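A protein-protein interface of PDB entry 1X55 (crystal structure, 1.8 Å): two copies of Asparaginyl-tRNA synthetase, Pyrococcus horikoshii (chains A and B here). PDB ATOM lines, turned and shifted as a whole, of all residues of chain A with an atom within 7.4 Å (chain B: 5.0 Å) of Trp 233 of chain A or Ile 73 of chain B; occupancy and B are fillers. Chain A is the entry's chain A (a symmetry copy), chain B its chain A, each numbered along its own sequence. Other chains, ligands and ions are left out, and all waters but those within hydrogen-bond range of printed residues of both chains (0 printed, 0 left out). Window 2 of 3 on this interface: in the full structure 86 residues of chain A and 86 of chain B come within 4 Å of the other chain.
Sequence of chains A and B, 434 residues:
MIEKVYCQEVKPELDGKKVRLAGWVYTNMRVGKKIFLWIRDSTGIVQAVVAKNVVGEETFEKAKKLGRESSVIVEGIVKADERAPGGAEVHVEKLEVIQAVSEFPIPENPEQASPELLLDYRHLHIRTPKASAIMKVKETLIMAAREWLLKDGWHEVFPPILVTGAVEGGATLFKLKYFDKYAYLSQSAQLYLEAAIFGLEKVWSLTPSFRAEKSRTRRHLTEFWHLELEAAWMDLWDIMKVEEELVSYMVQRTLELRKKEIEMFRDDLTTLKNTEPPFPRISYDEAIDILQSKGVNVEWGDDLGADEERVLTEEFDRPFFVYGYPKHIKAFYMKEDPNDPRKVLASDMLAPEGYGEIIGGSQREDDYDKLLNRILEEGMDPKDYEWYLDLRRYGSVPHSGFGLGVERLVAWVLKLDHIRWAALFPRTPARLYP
Trp 24 of chain B touches Ile 197 of chain A. NE1 of Trp 233 of chain A touches CD of Lys 4 of chain B, 3.9 Å away. Ala 22 of chain B touches Trp 233 of chain A. Trp 233 of chain A touches Gly 23 of chain B. CZ2 of Trp 233 of chain A touches CH2 of Trp 24 of chain B (3.9 Å). Trp 233 of chain A touches Ile 73 of chain B (CZ3 to CD1, 3.6 Å). CD1 of Ile 98 of chain B touches CZ3 of Trp 233 of chain A (3.6 Å). Gly 395 of chain A touches Ser 71 of chain B. Ser 396 of chain A touches Ile 98 of chain B (O to CG2, 3.2 Å). Ser 71 of chain B touches Val 397 of chain A (CB to CG1, 3.7 Å).
Of chain B, only Lys 4 (3.9 Å), Ala 22 (3.4 Å), Gly 23 (3.4 Å), Trp 24 (3.9 Å), Ile 73 (3.6 Å) and Ile 98 (3.6 Å) come within 4 Å of Trp 233 of chain A. Of chain A, only Trp 233 (3.6 Å) comes within 4 Å of Ile 73 of chain B. Printed residues of chain B within 4 Å of Ile 197 of chain A: Trp 24. Printed residues of chain B within 4 Å of Glu 201 of chain A: Lys 4 (2.8 Å). The nearest residue of chain A that does not touch Ile 73 of chain B is Val 397 of chain A (6.7 Å).
Of the 17 printed residues of chain A, 7 touch a printed residue of chain B. Hydrophobic or aromatic side chains of chain A that line the printed part of chain B: Trp 233 and Val 397. Of the 16 printed residues of chain B, 8 touch a printed residue of chain A. Hydrophobic or aromatic side chains of chain B within 4 Å of the printed part of chain A: Met 1, Ala 22, Trp 24, Ile 73 and Ile 98. Among the printed residues, 15 pairs touch across the chains.
The side-chain amino group (NZ) of Lys 4 of chain B is in hydrogen-bond range of the backbone carbonyl oxygen (O) of Ala 22 of chain B (2.8 Å). The backbone carbonyl oxygen (O) of Gly 23 of chain B is in hydrogen-bond range of the backbone NH (N) of Val 72 of chain B, at 2.9 Å. O of Ser 71 of chain B sits at hydrogen-bond distance from N of Ile 98 of chain B, 2.8 Å away. OE2 of Glu 201 of chain A lies within hydrogen-bond range of NE1 of Trp 233 of chain A. O of Pro 398 of chain A sits at hydrogen-bond distance from N of Trp 233 of chain A, at 2.8 Å. OD1 of Asp 238 of chain A is in hydrogen-bond range of N of Asp 235 of chain A (2.9 Å).
No position is printed for both chains. Of the 15 pairs that touch across the chains among the printed residues, none has its exchanged pair printed and touching as well.
OD2 of Asp 238 of chain A is in hydrogen-bond range of N of Met 1 of chain B, 2.8 Å away. NZ of Lys 4 of chain B is in salt-bridge range of OE2 of Glu 201 of chain A. The backbone carbonyl oxygen of Gly 395 of chain A lies within hydrogen-bond range of the indole nitrogen of Trp 24 of chain B, at 3.0 Å. OG of Ser 71 of chain B lies within hydrogen-bond range of O of Ser 396 of chain A (2.7 Å).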
ATOM      1  N   ILE A 197      -2.116  -0.261   0.322  1.00  0.00           N
ATOM      2  CA  ILE A 197      -0.951  -1.168   0.135  1.00  0.00           C
ATOM      3  C   ILE A 197      -1.378  -2.618  -0.130  1.00  0.00           C
ATOM      4  O   ILE A 197      -0.624  -3.382  -0.729  1.00  0.00           O
ATOM      5  CB  ILE A 197       0.068  -1.126   1.324  1.00  0.00           C
ATOM      6  CG1 ILE A 197      -0.587  -1.614   2.637  1.00  0.00           C
ATOM      7  CG2 ILE A 197       0.737   0.261   1.437  1.00  0.00           C
ATOM      8  CD1 ILE A 197       0.390  -1.745   3.834  1.00  0.00           C
ATOM      9  N   GLU A 201       0.747  -2.403  -2.911  1.00  0.00           N
ATOM     10  CA  GLU A 201       2.019  -2.646  -2.181  1.00  0.00           C
ATOM     11  C   GLU A 201       2.845  -1.413  -1.800  1.00  0.00           C
ATOM     12  O   GLU A 201       3.212  -1.256  -0.630  1.00  0.00           O
ATOM     13  CB  GLU A 201       2.927  -3.708  -2.848  1.00  0.00           C
ATOM     14  CG  GLU A 201       2.341  -5.119  -2.903  1.00  0.00           C
ATOM     15  CD  GLU A 201       3.330  -6.079  -3.545  1.00  0.00           C
ATOM     16  OE1 GLU A 201       3.233  -6.313  -4.784  1.00  0.00           O
ATOM     17  OE2 GLU A 201       4.247  -6.531  -2.818  1.00  0.00           O
ATOM     18  N   LYS A 202       3.200  -0.591  -2.784  1.00  0.00           N
ATOM     19  CA  LYS A 202       3.990   0.621  -2.539  1.00  0.00           C
ATOM     20  C   LYS A 202       3.167   1.806  -3.061  1.00  0.00           C
ATOM     21  O   LYS A 202       2.906   1.924  -4.271  1.00  0.00           O
ATOM     22  CB  LYS A 202       5.355   0.522  -3.223  1.00  0.00           C
ATOM     23  CG  LYS A 202       6.277  -0.522  -2.584  1.00  0.00           C
ATOM     24  CD  LYS A 202       7.533  -0.856  -3.449  1.00  0.00           C
ATOM     25  CE  LYS A 202       8.361   0.362  -3.804  1.00  0.00           C
ATOM     26  NZ  LYS A 202       9.749   0.000  -4.291  1.00  0.00           N
ATOM     27  N   ALA A 231       4.290   1.406   2.607  1.00  0.00           N
ATOM     28  CA  ALA A 231       4.770   0.224   1.893  1.00  0.00           C
ATOM     29  C   ALA A 231       4.571  -1.044   2.683  1.00  0.00           C
ATOM     30  O   ALA A 231       5.019  -1.160   3.824  1.00  0.00           O
ATOM     31  CB  ALA A 231       6.267   0.378   1.466  1.00  0.00           C
ATOM     32  N   ALA A 232       3.898  -2.006   2.051  1.00  0.00           N
ATOM     33  CA  ALA A 232       3.875  -3.379   2.546  1.00  0.00           C
ATOM     34  C   ALA A 232       5.301  -3.920   2.689  1.00  0.00           C
ATOM     35  O   ALA A 232       6.193  -3.533   1.930  1.00  0.00           O
ATOM     36  CB  ALA A 232       3.081  -4.262   1.573  1.00  0.00           C
ATOM     37  N   TRP A 233       5.491  -4.826   3.655  1.00  0.00           N
ATOM     38  CA  TRP A 233       6.710  -5.625   3.847  1.00  0.00           C
ATOM     39  C   TRP A 233       7.846  -4.865   4.557  1.00  0.00           C
ATOM     40  O   TRP A 233       8.712  -5.496   5.189  1.00  0.00           O
ATOM     41  CB  TRP A 233       7.223  -6.277   2.556  1.00  0.00           C
ATOM     42  CG  TRP A 233       6.138  -6.828   1.664  1.00  0.00           C
ATOM     43  CD1 TRP A 233       5.812  -6.380   0.425  1.00  0.00           C
ATOM     44  CD2 TRP A 233       5.236  -7.903   1.956  1.00  0.00           C
ATOM     45  NE1 TRP A 233       4.767  -7.113  -0.083  1.00  0.00           N
ATOM     46  CE2 TRP A 233       4.390  -8.050   0.841  1.00  0.00           C
ATOM     47  CE3 TRP A 233       5.058  -8.763   3.049  1.00  0.00           C
ATOM     48  CZ2 TRP A 233       3.388  -9.022   0.777  1.00  0.00           C
ATOM     49  CZ3 TRP A 233       4.060  -9.738   2.989  1.00  0.00           C
ATOM     50  CH2 TRP A 233       3.229  -9.849   1.861  1.00  0.00           C
ATOM     51  N   MET A 234       7.822  -3.535   4.500  1.00  0.00           N
ATOM     52  CA  MET A 234       8.925  -2.699   5.012  1.00  0.00           C
ATOM     53  C   MET A 234       8.802  -2.477   6.487  1.00  0.00           C
ATOM     54  O   MET A 234       7.704  -2.172   6.967  1.00  0.00           O
ATOM     55  CB  MET A 234       8.887  -1.330   4.337  1.00  0.00           C
ATOM     56  CG  MET A 234       9.302  -1.405   2.892  1.00  0.00           C
ATOM     57  SD  MET A 234       9.859   0.175   2.248  1.00  0.00           S
ATOM     58  CE  MET A 234       9.966  -0.210   0.523  1.00  0.00           C
ATOM     59  N   ASP A 235       9.923  -2.596   7.204  1.00  0.00           N
ATOM     60  CA  ASP A 235       9.957  -2.229   8.622  1.00  0.00           C
ATOM     61  C   ASP A 235      10.483  -0.804   8.768  1.00  0.00           C
ATOM     62  O   ASP A 235      10.668  -0.086   7.776  1.00  0.00           O
ATOM     63  CB  ASP A 235      10.771  -3.229   9.469  1.00  0.00           C
ATOM     64  CG  ASP A 235      12.209  -3.310   9.077  1.00  0.00           C
ATOM     65  OD1 ASP A 235      12.761  -2.373   8.441  1.00  0.00           O
ATOM     66  OD2 ASP A 235      12.894  -4.335   9.358  1.00  0.00           O
ATOM     67  N   LEU A 236      10.703  -0.385  10.002  1.00  0.00           N
ATOM     68  CA  LEU A 236      11.149   0.995  10.250  1.00  0.00           C
ATOM     69  C   LEU A 236      12.455   1.315   9.528  1.00  0.00           C
ATOM     70  O   LEU A 236      12.579   2.385   8.920  1.00  0.00           O
ATOM     71  CB  LEU A 236      11.274   1.228  11.762  1.00  0.00           C
ATOM     72  CG  LEU A 236      11.884   2.574  12.176  1.00  0.00           C
ATOM     73  CD1 LEU A 236      10.957   3.750  11.819  1.00  0.00           C
ATOM     74  CD2 LEU A 236      12.167   2.565  13.644  1.00  0.00           C
ATOM     75  N   ASP A 238      13.806  -0.102   6.941  1.00  0.00           N
ATOM     76  CA  ASP A 238      13.510  -0.036   5.521  1.00  0.00           C
ATOM     77  C   ASP A 238      12.942   1.326   5.150  1.00  0.00           C
ATOM     78  O   ASP A 238      13.392   1.936   4.169  1.00  0.00           O
ATOM     79  CB  ASP A 238      12.452  -1.087   5.167  1.00  0.00           C
ATOM     80  CG  ASP A 238      12.967  -2.497   5.315  1.00  0.00           C
ATOM     81  OD1 ASP A 238      12.122  -3.397   5.498  1.00  0.00           O
ATOM     82  OD2 ASP A 238      14.189  -2.773   5.257  1.00  0.00           O
ATOM     83  N   GLN A 363       6.980   2.347  11.628  1.00  0.00           N
ATOM     84  CA  GLN A 363       6.352   1.073  11.352  1.00  0.00           C
ATOM     85  C   GLN A 363       4.978   1.018  12.038  1.00  0.00           C
ATOM     86  O   GLN A 363       4.778   1.588  13.115  1.00  0.00           O
ATOM     87  CB  GLN A 363       7.267  -0.068  11.837  1.00  0.00           C
ATOM     88  CG  GLN A 363       6.766  -1.436  11.424  1.00  0.00           C
ATOM     89  CD  GLN A 363       7.815  -2.529  11.559  1.00  0.00           C
ATOM     90  OE1 GLN A 363       8.966  -2.254  11.876  1.00  0.00           O
ATOM     91  NE2 GLN A 363       7.423  -3.763  11.276  1.00  0.00           N
ATOM     92  N   GLY A 395      -5.500 -10.602   6.215  1.00  0.00           N
ATOM     93  CA  GLY A 395      -4.209 -10.759   5.579  1.00  0.00           C
ATOM     94  C   GLY A 395      -3.222  -9.669   5.958  1.00  0.00           C
ATOM     95  O   GLY A 395      -2.529  -9.112   5.092  1.00  0.00           O
ATOM     96  N   SER A 396      -3.140  -9.394   7.254  1.00  0.00           N
ATOM     97  CA  SER A 396      -2.175  -8.437   7.801  1.00  0.00           C
ATOM     98  C   SER A 396      -0.746  -8.743   7.324  1.00  0.00           C
ATOM     99  O   SER A 396      -0.349  -9.906   7.162  1.00  0.00           O
ATOM    100  CB  SER A 396      -2.243  -8.415   9.342  1.00  0.00           C
ATOM    101  OG  SER A 396      -1.482  -7.347   9.883  1.00  0.00           O
ATOM    102  N   VAL A 397       0.000  -7.683   7.044  1.00  0.00           N
ATOM    103  CA  VAL A 397       1.424  -7.795   6.713  1.00  0.00           C
ATOM    104  C   VAL A 397       2.173  -6.689   7.469  1.00  0.00           C
ATOM    105  O   VAL A 397       1.573  -5.647   7.767  1.00  0.00           O
ATOM    106  CB  VAL A 397       1.689  -7.650   5.174  1.00  0.00           C
ATOM    107  CG1 VAL A 397       0.919  -8.731   4.346  1.00  0.00           C
ATOM    108  CG2 VAL A 397       1.317  -6.247   4.683  1.00  0.00           C
ATOM    109  N   PRO A 398       3.456  -6.894   7.792  1.00  0.00           N
ATOM    110  CA  PRO A 398       4.247  -5.792   8.395  1.00  0.00           C
ATOM    111  C   PRO A 398       4.272  -4.654   7.374  1.00  0.00           C
ATOM    112  O   PRO A 398       4.339  -4.921   6.162  1.00  0.00           O
ATOM    113  CB  PRO A 398       5.678  -6.369   8.541  1.00  0.00           C
ATOM    114  CG  PRO A 398       5.673  -7.739   7.838  1.00  0.00           C
ATOM    115  CD  PRO A 398       4.235  -8.138   7.626  1.00  0.00           C
ATOM    116  N   HIS A 399       4.189  -3.414   7.837  1.00  0.00           N
ATOM    117  CA  HIS A 399       4.264  -2.267   6.920  1.00  0.00           C
ATOM    118  C   HIS A 399       4.598  -0.994   7.679  1.00  0.00           C
ATOM    119  O   HIS A 399       4.422  -0.927   8.896  1.00  0.00           O
ATOM    120  CB  HIS A 399       2.965  -2.115   6.092  1.00  0.00           C
ATOM    121  CG  HIS A 399       1.740  -1.855   6.920  1.00  0.00           C
ATOM    122  ND1 HIS A 399       1.054  -2.858   7.574  1.00  0.00           N
ATOM    123  CD2 HIS A 399       1.054  -0.711   7.159  1.00  0.00           C
ATOM    124  CE1 HIS A 399       0.019  -2.333   8.214  1.00  0.00           C
ATOM    125  NE2 HIS A 399       0.000  -1.032   7.985  1.00  0.00           N
ATOM    126  N   SER A 400       5.092  -0.003   6.934  1.00  0.00           N
ATOM    127  CA  SER A 400       5.652   1.232   7.477  1.00  0.00           C
ATOM    128  C   SER A 400       5.433   2.348   6.461  1.00  0.00           C
ATOM    129  O   SER A 400       5.231   2.095   5.260  1.00  0.00           O
ATOM    130  CB  SER A 400       7.159   1.100   7.693  1.00  0.00           C
ATOM    131  OG  SER A 400       7.468   0.031   8.575  1.00  0.00           O
ATOM    132  N   MET B   1      15.447  -5.225   4.598  1.00  0.00           N
ATOM    133  CA  MET B   1      14.351  -6.119   4.137  1.00  0.00           C
ATOM    134  C   MET B   1      14.899  -7.268   3.308  1.00  0.00           C
ATOM    135  O   MET B   1      15.833  -7.085   2.518  1.00  0.00           O
ATOM    136  CB  MET B   1      13.365  -5.322   3.283  1.00  0.00           C
ATOM    137  CG  MET B   1      12.220  -6.122   2.670  1.00  0.00           C
ATOM    138  SD  MET B   1      11.076  -5.047   1.781  1.00  0.00           S
ATOM    139  CE  MET B   1      12.194  -3.838   1.031  1.00  0.00           C
ATOM    140  N   LYS B   4      11.841  -9.362  -2.227  1.00  0.00           N
ATOM    141  CA  LYS B   4      10.868 -10.244  -2.853  1.00  0.00           C
ATOM    142  C   LYS B   4      11.004 -10.199  -4.364  1.00  0.00           C
ATOM    143  O   LYS B   4      11.601  -9.278  -4.934  1.00  0.00           O
ATOM    144  CB  LYS B   4       9.439  -9.891  -2.427  1.00  0.00           C
ATOM    145  CG  LYS B   4       9.008  -8.447  -2.755  1.00  0.00           C
ATOM    146  CD  LYS B   4       7.480  -8.263  -2.699  1.00  0.00           C
ATOM    147  CE  LYS B   4       6.782  -8.935  -3.928  1.00  0.00           C
ATOM    148  NZ  LYS B   4       5.262  -8.925  -3.822  1.00  0.00           N
ATOM    149  N   ARG B  20      11.476 -15.618  -3.806  1.00  0.00           N
ATOM    150  CA  ARG B  20      10.688 -15.409  -2.603  1.00  0.00           C
ATOM    151  C   ARG B  20       9.520 -14.558  -3.027  1.00  0.00           C
ATOM    152  O   ARG B  20       9.689 -13.373  -3.352  1.00  0.00           O
ATOM    153  CB  ARG B  20      11.528 -14.663  -1.558  1.00  0.00           C
ATOM    154  CG  ARG B  20      10.855 -14.318  -0.255  1.00  0.00           C
ATOM    155  CD  ARG B  20      11.914 -13.956   0.782  1.00  0.00           C
ATOM    156  NE  ARG B  20      11.415 -13.303   1.983  1.00  0.00           N
ATOM    157  CZ  ARG B  20      11.283 -13.912   3.172  1.00  0.00           C
ATOM    158  NH1 ARG B  20      11.577 -15.204   3.306  1.00  0.00           N
ATOM    159  NH2 ARG B  20      10.848 -13.230   4.229  1.00  0.00           N
ATOM    160  N   LEU B  21       8.338 -15.167  -3.067  1.00  0.00           N
ATOM    161  CA  LEU B  21       7.115 -14.409  -3.297  1.00  0.00           C
ATOM    162  C   LEU B  21       6.604 -13.862  -1.969  1.00  0.00           C
ATOM    163  O   LEU B  21       6.797 -14.472  -0.919  1.00  0.00           O
ATOM    164  CB  LEU B  21       6.039 -15.308  -3.899  1.00  0.00           C
ATOM    165  CG  LEU B  21       6.389 -16.141  -5.134  1.00  0.00           C
ATOM    166  CD1 LEU B  21       5.157 -16.931  -5.532  1.00  0.00           C
ATOM    167  CD2 LEU B  21       6.857 -15.239  -6.273  1.00  0.00           C
ATOM    168  N   ALA B  22       5.896 -12.738  -2.022  1.00  0.00           N
ATOM    169  CA  ALA B  22       5.238 -12.190  -0.845  1.00  0.00           C
ATOM    170  C   ALA B  22       3.918 -11.583  -1.328  1.00  0.00           C
ATOM    171  O   ALA B  22       3.903 -10.774  -2.263  1.00  0.00           O
ATOM    172  CB  ALA B  22       6.125 -11.120  -0.164  1.00  0.00           C
ATOM    173  N   GLY B  23       2.815 -12.026  -0.738  1.00  0.00           N
ATOM    174  CA  GLY B  23       1.508 -11.581  -1.185  1.00  0.00           C
ATOM    175  C   GLY B  23       0.361 -12.287  -0.508  1.00  0.00           C
ATOM    176  O   GLY B  23       0.459 -12.684   0.659  1.00  0.00           O
ATOM    177  N   TRP B  24      -0.743 -12.402  -1.242  1.00  0.00           N
ATOM    178  CA  TRP B  24      -2.015 -12.818  -0.678  1.00  0.00           C
ATOM    179  C   TRP B  24      -2.617 -13.940  -1.519  1.00  0.00           C
ATOM    180  O   TRP B  24      -2.510 -13.923  -2.754  1.00  0.00           O
ATOM    181  CB  TRP B  24      -2.978 -11.617  -0.609  1.00  0.00           C
ATOM    182  CG  TRP B  24      -2.466 -10.534   0.329  1.00  0.00           C
ATOM    183  CD1 TRP B  24      -2.732 -10.399   1.658  1.00  0.00           C
ATOM    184  CD2 TRP B  24      -1.612  -9.449  -0.021  1.00  0.00           C
ATOM    185  NE1 TRP B  24      -2.084  -9.297   2.169  1.00  0.00           N
ATOM    186  CE2 TRP B  24      -1.371  -8.703   1.156  1.00  0.00           C
ATOM    187  CE3 TRP B  24      -0.979  -9.049  -1.216  1.00  0.00           C
ATOM    188  CZ2 TRP B  24      -0.554  -7.562   1.174  1.00  0.00           C
ATOM    189  CZ3 TRP B  24      -0.136  -7.910  -1.197  1.00  0.00           C
ATOM    190  CH2 TRP B  24       0.064  -7.184  -0.014  1.00  0.00           C
ATOM    191  N   SER B  71      -2.320 -13.875   4.043  1.00  0.00           N
ATOM    192  CA  SER B  71      -1.038 -13.259   3.730  1.00  0.00           C
ATOM    193  C   SER B  71       0.077 -14.284   3.932  1.00  0.00           C
ATOM    194  O   SER B  71       0.152 -14.961   4.976  1.00  0.00           O
ATOM    195  CB  SER B  71      -0.810 -11.997   4.540  1.00  0.00           C
ATOM    196  OG  SER B  71      -1.038 -12.224   5.917  1.00  0.00           O
ATOM    197  N   VAL B  72       0.905 -14.421   2.906  1.00  0.00           N
ATOM    198  CA  VAL B  72       1.910 -15.471   2.866  1.00  0.00           C
ATOM    199  C   VAL B  72       3.272 -15.011   2.313  1.00  0.00           C
ATOM    200  O   VAL B  72       3.353 -14.097   1.458  1.00  0.00           O
ATOM    201  CB  VAL B  72       1.438 -16.689   2.003  1.00  0.00           C
ATOM    202  CG1 VAL B  72       0.314 -17.436   2.677  1.00  0.00           C
ATOM    203  CG2 VAL B  72       1.023 -16.250   0.610  1.00  0.00           C
ATOM    204  N   ILE B  73       4.327 -15.671   2.781  1.00  0.00           N
ATOM    205  CA  ILE B  73       5.634 -15.608   2.131  1.00  0.00           C
ATOM    206  C   ILE B  73       5.929 -17.000   1.615  1.00  0.00           C
ATOM    207  O   ILE B  73       5.786 -17.990   2.356  1.00  0.00           O
ATOM    208  CB  ILE B  73       6.766 -15.192   3.110  1.00  0.00           C
ATOM    209  CG1 ILE B  73       6.385 -13.928   3.895  1.00  0.00           C
ATOM    210  CG2 ILE B  73       8.088 -15.038   2.362  1.00  0.00           C
ATOM    211  CD1 ILE B  73       6.123 -12.746   3.001  1.00  0.00           C
ATOM    212  N   VAL B  74       6.308 -17.072   0.345  1.00  0.00           N
ATOM    213  CA  VAL B  74       6.533 -18.345  -0.327  1.00  0.00           C
ATOM    214  C   VAL B  74       7.939 -18.380  -0.918  1.00  0.00           C
ATOM    215  O   VAL B  74       8.275 -17.543  -1.763  1.00  0.00           O
ATOM    216  CB  VAL B  74       5.454 -18.546  -1.455  1.00  0.00           C
ATOM    217  CG1 VAL B  74       5.755 -19.757  -2.293  1.00  0.00           C
ATOM    218  CG2 VAL B  74       4.057 -18.637  -0.839  1.00  0.00           C
ATOM    219  N   GLU B  75       8.782 -19.316  -0.487  1.00  0.00           N
ATOM    220  CA  GLU B  75      10.052 -19.509  -1.192  1.00  0.00           C
ATOM    221  C   GLU B  75      10.055 -20.818  -1.969  1.00  0.00           C
ATOM    222  O   GLU B  75       9.570 -21.828  -1.478  1.00  0.00           O
ATOM    223  CB  GLU B  75      11.244 -19.478  -0.238  1.00  0.00           C
ATOM    224  CG  GLU B  75      11.363 -18.162   0.533  1.00  0.00           C
ATOM    225  CD  GLU B  75      12.500 -18.174   1.542  1.00  0.00           C
ATOM    226  OE1 GLU B  75      12.691 -17.139   2.240  1.00  0.00           O
ATOM    227  OE2 GLU B  75      13.196 -19.212   1.652  1.00  0.00           O
ATOM    228  N   LYS B  94       9.346 -23.585   0.933  1.00  0.00           N
ATOM    229  CA  LYS B  94       9.024 -23.057   2.251  1.00  0.00           C
ATOM    230  C   LYS B  94       7.778 -22.188   2.155  1.00  0.00           C
ATOM    231  O   LYS B  94       7.644 -21.409   1.218  1.00  0.00           O
ATOM    232  CB  LYS B  94      10.213 -22.251   2.803  1.00  0.00           C
ATOM    233  CG  LYS B  94      10.083 -21.803   4.250  1.00  0.00           C
ATOM    234  CD  LYS B  94       9.627 -20.337   4.369  1.00  0.00           C
ATOM    235  CE  LYS B  94       9.672 -19.803   5.834  1.00  0.00           C
ATOM    236  NZ  LYS B  94       8.675 -20.481   6.740  1.00  0.00           N
ATOM    237  N   LEU B  95       6.890 -22.326   3.138  1.00  0.00           N
ATOM    238  CA  LEU B  95       5.685 -21.515   3.197  1.00  0.00           C
ATOM    239  C   LEU B  95       5.600 -20.900   4.563  1.00  0.00           C
ATOM    240  O   LEU B  95       5.563 -21.632   5.553  1.00  0.00           O
ATOM    241  CB  LEU B  95       4.439 -22.376   2.913  1.00  0.00           C
ATOM    242  CG  LEU B  95       3.062 -21.734   3.055  1.00  0.00           C
ATOM    243  CD1 LEU B  95       2.938 -20.566   2.072  1.00  0.00           C
ATOM    244  CD2 LEU B  95       1.975 -22.776   2.800  1.00  0.00           C
ATOM    245  N   GLU B  96       5.613 -19.567   4.629  1.00  0.00           N
ATOM    246  CA  GLU B  96       5.337 -18.858   5.884  1.00  0.00           C
ATOM    247  C   GLU B  96       3.985 -18.193   5.832  1.00  0.00           C
ATOM    248  O   GLU B  96       3.728 -17.303   4.989  1.00  0.00           O
ATOM    249  CB  GLU B  96       6.408 -17.816   6.200  1.00  0.00           C
ATOM    250  CG  GLU B  96       6.106 -17.060   7.496  1.00  0.00           C
ATOM    251  CD  GLU B  96       7.048 -15.889   7.744  1.00  0.00           C
ATOM    252  OE1 GLU B  96       6.679 -15.011   8.573  1.00  0.00           O
ATOM    253  OE2 GLU B  96       8.147 -15.834   7.115  1.00  0.00           O
ATOM    254  N   ILE B  98       1.668 -15.677   7.205  1.00  0.00           N
ATOM    255  CA  ILE B  98       1.632 -14.493   8.063  1.00  0.00           C
ATOM    256  C   ILE B  98       0.282 -14.398   8.766  1.00  0.00           C
ATOM    257  O   ILE B  98       0.214 -14.363  10.007  1.00  0.00           O
ATOM    258  CB  ILE B  98       1.946 -13.198   7.279  1.00  0.00           C
ATOM    259  CG1 ILE B  98       3.307 -13.300   6.624  1.00  0.00           C
ATOM    260  CG2 ILE B  98       1.885 -11.981   8.227  1.00  0.00           C
ATOM    261  CD1 ILE B  98       3.593 -12.185   5.593  1.00  0.00           C
